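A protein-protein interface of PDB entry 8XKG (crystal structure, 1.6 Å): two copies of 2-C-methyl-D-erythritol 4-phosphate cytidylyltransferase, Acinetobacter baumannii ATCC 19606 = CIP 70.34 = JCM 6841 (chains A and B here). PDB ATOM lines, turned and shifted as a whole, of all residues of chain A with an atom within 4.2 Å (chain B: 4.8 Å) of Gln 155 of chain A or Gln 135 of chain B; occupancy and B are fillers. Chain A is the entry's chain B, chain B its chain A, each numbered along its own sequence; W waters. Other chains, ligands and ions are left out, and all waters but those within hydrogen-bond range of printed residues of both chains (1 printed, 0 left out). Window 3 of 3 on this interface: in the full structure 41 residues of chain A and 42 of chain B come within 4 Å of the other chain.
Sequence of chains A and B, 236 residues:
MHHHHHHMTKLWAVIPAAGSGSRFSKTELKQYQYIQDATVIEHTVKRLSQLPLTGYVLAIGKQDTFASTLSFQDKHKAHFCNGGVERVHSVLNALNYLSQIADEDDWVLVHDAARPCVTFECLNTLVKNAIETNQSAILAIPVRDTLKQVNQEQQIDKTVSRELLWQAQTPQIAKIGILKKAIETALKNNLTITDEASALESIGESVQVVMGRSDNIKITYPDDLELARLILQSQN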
ATOM      1  N   VAL A 150     -13.348 -26.349 -22.563  1.00  0.00           N
ATOM      2  CA  VAL A 150     -13.702 -24.942 -22.713  1.00  0.00           C
ATOM      3  C   VAL A 150     -12.576 -24.231 -23.446  1.00  0.00           C
ATOM      4  O   VAL A 150     -11.405 -24.359 -23.069  1.00  0.00           O
ATOM      5  CB  VAL A 150     -13.969 -24.282 -21.346  1.00  0.00           C
ATOM      6  CG1 VAL A 150     -14.238 -22.800 -21.507  1.00  0.00           C
ATOM      7  CG2 VAL A 150     -15.136 -24.966 -20.650  1.00  0.00           C
ATOM      8  N   ASN A 151     -12.929 -23.454 -24.463  1.00  0.00           N
ATOM      9  CA  ASN A 151     -11.923 -22.774 -25.263  1.00  0.00           C
ATOM     10  C   ASN A 151     -11.531 -21.442 -24.626  1.00  0.00           C
ATOM     11  O   ASN A 151     -12.077 -21.024 -23.602  1.00  0.00           O
ATOM     12  CB  ASN A 151     -12.405 -22.613 -26.717  1.00  0.00           C
ATOM     13  CG  ASN A 151     -13.501 -21.554 -26.897  1.00  0.00           C
ATOM     14  OD1 ASN A 151     -13.752 -20.717 -26.033  1.00  0.00           O
ATOM     15  ND2 ASN A 151     -14.150 -21.595 -28.056  1.00  0.00           N
ATOM     16  N   GLU A 153     -12.106 -18.526 -25.288  1.00  0.00           N
ATOM     17  CA  GLU A 153     -13.150 -17.558 -25.220  1.00  0.00           C
ATOM     18  C   GLU A 153     -14.259 -17.937 -24.177  1.00  0.00           C
ATOM     19  O   GLU A 153     -15.283 -17.340 -24.218  1.00  0.00           O
ATOM     20  CB  GLU A 153     -13.801 -17.456 -26.545  1.00  0.00           C
ATOM     21  CG  GLU A 153     -12.919 -16.911 -27.658  1.00  0.00           C
ATOM     22  CD  GLU A 153     -11.794 -17.810 -28.118  1.00  0.00           C
ATOM     23  OE1 GLU A 153     -10.637 -17.318 -28.215  1.00  0.00           O
ATOM     24  OE2 GLU A 153     -12.008 -19.005 -28.404  1.00  0.00           O
ATOM     25  N   GLN A 154     -13.960 -18.908 -23.331  1.00  0.00           N
ATOM     26  CA  GLN A 154     -14.887 -19.388 -22.303  1.00  0.00           C
ATOM     27  C   GLN A 154     -16.186 -19.922 -22.905  1.00  0.00           C
ATOM     28  O   GLN A 154     -17.254 -19.824 -22.298  1.00  0.00           O
ATOM     29  CB  GLN A 154     -15.157 -18.318 -21.237  1.00  0.00           C
ATOM     30  CG  GLN A 154     -13.911 -18.014 -20.395  1.00  0.00           C
ATOM     31  CD  GLN A 154     -14.206 -17.665 -18.942  1.00  0.00           C
ATOM     32  OE1 GLN A 154     -15.348 -17.411 -18.561  1.00  0.00           O
ATOM     33  NE2 GLN A 154     -13.160 -17.656 -18.120  1.00  0.00           N
ATOM     34  N   GLN A 155     -16.104 -20.454 -24.120  1.00  0.00           N
ATOM     35  CA  GLN A 155     -17.211 -21.149 -24.759  1.00  0.00           C
ATOM     36  C   GLN A 155     -16.963 -22.648 -24.623  1.00  0.00           C
ATOM     37  O   GLN A 155     -15.818 -23.101 -24.708  1.00  0.00           O
ATOM     38  CB  GLN A 155     -17.309 -20.766 -26.237  1.00  0.00           C
ATOM     39  CG  GLN A 155     -17.649 -19.304 -26.497  1.00  0.00           C
ATOM     40  CD  GLN A 155     -19.099 -18.977 -26.219  1.00  0.00           C
ATOM     41  OE1 GLN A 155     -19.419 -17.907 -25.701  1.00  0.00           O
ATOM     42  NE2 GLN A 155     -19.988 -19.896 -26.574  1.00  0.00           N
ATOM     43  N   ILE A 156     -18.029 -23.417 -24.422  1.00  0.00           N
ATOM     44  CA  ILE A 156     -17.888 -24.865 -24.292  1.00  0.00           C
ATOM     45  C   ILE A 156     -17.644 -25.480 -25.663  1.00  0.00           C
ATOM     46  O   ILE A 156     -18.396 -25.230 -26.611  1.00  0.00           O
ATOM     47  CB  ILE A 156     -19.128 -25.485 -23.628  1.00  0.00           C
ATOM     48  CG1 ILE A 156     -19.276 -25.000 -22.184  1.00  0.00           C
ATOM     49  CG2 ILE A 156     -19.060 -27.007 -23.689  1.00  0.00           C
ATOM     50  CD1 ILE A 156     -20.488 -25.569 -21.480  1.00  0.00           C
ATOM     51  N   ASP A 157     -16.671 -26.352 -25.779  1.00  0.00           N
ATOM     52  CA  ASP A 157     -16.413 -27.063 -27.053  1.00  0.00           C
ATOM     53  C   ASP A 157     -17.211 -28.337 -26.993  1.00  0.00           C
ATOM     54  O   ASP A 157     -17.895 -28.654 -27.916  1.00  0.00           O
ATOM     55  CB  ASP A 157     -14.942 -27.439 -27.211  1.00  0.00           C
ATOM     56  CG  ASP A 157     -14.063 -26.296 -27.591  1.00  0.00           C
ATOM     57  OD1 ASP A 157     -14.512 -25.368 -28.244  1.00  0.00           O
ATOM     58  OD2 ASP A 157     -12.871 -26.319 -27.234  1.00  0.00           O
ATOM     59  N   TRP B 107     -36.281 -16.742 -20.395  1.00  0.00           N
ATOM     60  CA  TRP B 107     -35.118 -17.486 -19.926  1.00  0.00           C
ATOM     61  C   TRP B 107     -35.479 -18.377 -18.748  1.00  0.00           C
ATOM     62  O   TRP B 107     -36.277 -17.994 -17.888  1.00  0.00           O
ATOM     63  CB  TRP B 107     -33.993 -16.537 -19.524  1.00  0.00           C
ATOM     64  CG  TRP B 107     -33.487 -15.752 -20.670  1.00  0.00           C
ATOM     65  CD1 TRP B 107     -34.048 -14.637 -21.202  1.00  0.00           C
ATOM     66  CD2 TRP B 107     -32.334 -16.042 -21.463  1.00  0.00           C
ATOM     67  NE1 TRP B 107     -33.303 -14.190 -22.264  1.00  0.00           N
ATOM     68  CE2 TRP B 107     -32.246 -15.041 -22.449  1.00  0.00           C
ATOM     69  CE3 TRP B 107     -31.364 -17.047 -21.431  1.00  0.00           C
ATOM     70  CZ2 TRP B 107     -31.223 -15.012 -23.391  1.00  0.00           C
ATOM     71  CZ3 TRP B 107     -30.352 -17.019 -22.369  1.00  0.00           C
ATOM     72  CH2 TRP B 107     -30.288 -16.009 -23.336  1.00  0.00           C
ATOM     73  N   ALA B 130     -25.861 -14.129 -19.885  1.00  0.00           N
ATOM     74  CA  ALA B 130     -26.736 -14.792 -20.844  1.00  0.00           C
ATOM     75  C   ALA B 130     -27.619 -13.785 -21.566  1.00  0.00           C
ATOM     76  O   ALA B 130     -27.740 -13.819 -22.796  1.00  0.00           O
ATOM     77  CB  ALA B 130     -27.585 -15.849 -20.138  1.00  0.00           C
ATOM     78  N   THR B 133     -25.356 -11.421 -23.995  1.00  0.00           N
ATOM     79  CA  THR B 133     -24.845 -12.124 -25.156  1.00  0.00           C
ATOM     80  C   THR B 133     -25.949 -12.804 -25.941  1.00  0.00           C
ATOM     81  O   THR B 133     -25.700 -13.245 -27.067  1.00  0.00           O
ATOM     82  CB  THR B 133     -23.811 -13.162 -24.734  1.00  0.00           C
ATOM     83  OG1 THR B 133     -24.445 -14.146 -23.909  1.00  0.00           O
ATOM     84  CG2 THR B 133     -22.682 -12.504 -23.956  1.00  0.00           C
ATOM     85  N   ASN B 134     -27.153 -12.891 -25.374  1.00  0.00           N
ATOM     86  CA  ASN B 134     -28.270 -13.600 -25.990  1.00  0.00           C
ATOM     87  C   ASN B 134     -27.933 -15.068 -26.250  1.00  0.00           C
ATOM     88  O   ASN B 134     -28.380 -15.653 -27.239  1.00  0.00           O
ATOM     89  CB  ASN B 134     -28.712 -12.900 -27.280  1.00  0.00           C
ATOM     90  CG  ASN B 134     -30.092 -13.319 -27.725  1.00  0.00           C
ATOM     91  OD1 ASN B 134     -31.010 -13.430 -26.915  1.00  0.00           O
ATOM     92  ND2 ASN B 134     -30.247 -13.551 -29.022  1.00  0.00           N
ATOM     93  N   GLN B 135     -27.146 -15.678 -25.361  1.00  0.00           N
ATOM     94  CA  GLN B 135     -26.735 -17.067 -25.512  1.00  0.00           C
ATOM     95  C   GLN B 135     -26.793 -17.772 -24.163  1.00  0.00           C
ATOM     96  O   GLN B 135     -26.717 -17.142 -23.104  1.00  0.00           O
ATOM     97  CB  GLN B 135     -25.311 -17.199 -26.081  1.00  0.00           C
ATOM     98  CG  GLN B 135     -25.059 -16.485 -27.401  1.00  0.00           C
ATOM     99  CD  GLN B 135     -23.646 -16.697 -27.923  1.00  0.00           C
ATOM    100  OE1 GLN B 135     -22.692 -16.801 -27.150  1.00  0.00           O
ATOM    101  NE2 GLN B 135     -23.508 -16.763 -29.242  1.00  0.00           N
ATOM    102  N   SER B 136     -26.897 -19.098 -24.222  1.00  0.00           N
ATOM    103  CA  SER B 136     -26.954 -19.924 -23.024  1.00  0.00           C
ATOM    104  C   SER B 136     -25.645 -19.833 -22.241  1.00  0.00           C
ATOM    105  O   SER B 136     -24.587 -19.504 -22.783  1.00  0.00           O
ATOM    106  CB  SER B 136     -27.235 -21.382 -23.390  1.00  0.00           C
ATOM    107  OG  SER B 136     -28.322 -21.486 -24.294  1.00  0.00           O
ATOM    108  N   ALA B 137     -25.725 -20.146 -20.949  1.00  0.00           N
ATOM    109  CA  ALA B 137     -24.553 -20.064 -20.089  1.00  0.00           C
ATOM    110  C   ALA B 137     -24.716 -21.003 -18.903  1.00  0.00           C
ATOM    111  O   ALA B 137     -25.830 -21.389 -18.540  1.00  0.00           O
ATOM    112  CB  ALA B 137     -24.316 -18.630 -19.603  1.00  0.00           C
ATOM    113  N   SER B 206     -24.349 -22.477 -28.836  1.00  0.00           N
ATOM    114  CA  SER B 206     -23.202 -22.048 -28.049  1.00  0.00           C
ATOM    115  C   SER B 206     -23.590 -21.938 -26.580  1.00  0.00           C
ATOM    116  O   SER B 206     -24.696 -21.508 -26.246  1.00  0.00           O
ATOM    117  CB  SER B 206     -22.676 -20.703 -28.550  1.00  0.00           C
ATOM    118  OG  SER B 206     -22.183 -20.804 -29.873  1.00  0.00           O
ATOM    119  N   VAL B 207     -22.680 -22.344 -25.698  1.00  0.00           N
ATOM    120  CA  VAL B 207     -22.887 -22.236 -24.259  1.00  0.00           C
ATOM    121  C   VAL B 207     -21.646 -21.588 -23.667  1.00  0.00           C
ATOM    122  O   VAL B 207     -20.535 -22.111 -23.826  1.00  0.00           O
ATOM    123  CB  VAL B 207     -23.152 -23.603 -23.601  1.00  0.00           C
ATOM    124  CG1 VAL B 207     -23.360 -23.443 -22.098  1.00  0.00           C
ATOM    125  CG2 VAL B 207     -24.348 -24.288 -24.246  1.00  0.00           C
ATOM    126  N   GLN B 208     -21.830 -20.468 -22.973  1.00  0.00           N
ATOM    127  CA  GLN B 208     -20.715 -19.758 -22.355  1.00  0.00           C
ATOM    128  C   GLN B 208     -20.563 -20.120 -20.880  1.00  0.00           C
ATOM    129  O   GLN B 208     -21.551 -20.246 -20.157  1.00  0.00           O
ATOM    130  CB  GLN B 208     -20.894 -18.247 -22.510  1.00  0.00           C
ATOM    131  CG  GLN B 208     -19.705 -17.427 -22.033  1.00  0.00           C
ATOM    132  CD  GLN B 208     -20.028 -15.952 -21.904  1.00  0.00           C
ATOM    133  OE1 GLN B 208     -21.080 -15.493 -22.350  1.00  0.00           O
ATOM    134  NE2 GLN B 208     -19.123 -15.200 -21.288  1.00  0.00           N
HETATM  135  O   HOH W   1     -20.394 -23.411 -27.085  1.00  0.00           O
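O of Val 207 of chain B lies within hydrogen-bond range of N of Ile 156 of chain A.
OD1 of Asn 151 of chain A is in hydrogen-bond range of N of Gln 155 of chain A (3.0 Å). The side-chain amide oxygen (OD1) of Asn 151 of chain A sits at hydrogen-bond distance from the backbone NH (N) of Gln 154 of chain A (3.3 Å). OG1 of Thr 133 of chain B lies close to N of Gln 135 of chain B, at 3.4 Å. The backbone carbonyl oxygen of Ser 136 of chain B sits at hydrogen-bond distance from the backbone NH of Gln 208 of chain B, at 2.9 Å. The backbone carbonyl oxygen (O) of Ala 130 of chain B sits at hydrogen-bond distance from the backbone NH (N) of Gln 135 of chain B.
Gln 208 of chain B touches Gln 154 of chain A (CG to O, 3.4 Å). Gln 135 of chain B touches Gln 155 of chain A. Gln 155 of chain A touches Ser 206 of chain B (NE2 to CB, 3.4 Å). Gln 155 of chain A touches Val 207 of chain B. Gln 208 of chain B touches Gln 155 of chain A (CB to OE1, 3.5 Å).
Printed residues of chain B within 4 Å of Gln 154 of chain A: Gln 208. Of chain B, only Gln 135, Ser 206, Val 207 and Gln 208 come within 4 Å of Gln 155 of chain A. Of the printed residues of chain B, Ile 156 of chain A touches Val 207 (2.9 Å). Gln 135 of chain B touches just one residue of chain A: Gln 155. Printed residues of chain A within 4 Å of Val 207 of chain B: Gln 155 and Ile 156. Of the printed residues of chain A, Gln 208 of chain B touches Gln 154 and Gln 155. The nearest printed residue of chain A that does not touch Ser 206 of chain B is Ile 156 of chain A (5.9 Å).
Among the printed residues, 6 pairs touch across the chains.
No position is printed for both chains. Of the 6 pairs that touch across the chains among the printed residues, none has its exchanged pair printed and touching as well.
Water W1 bridges O of Ile 156 of chain A (2.7 Å) and N of Val 207 of chain B (2.9 Å).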
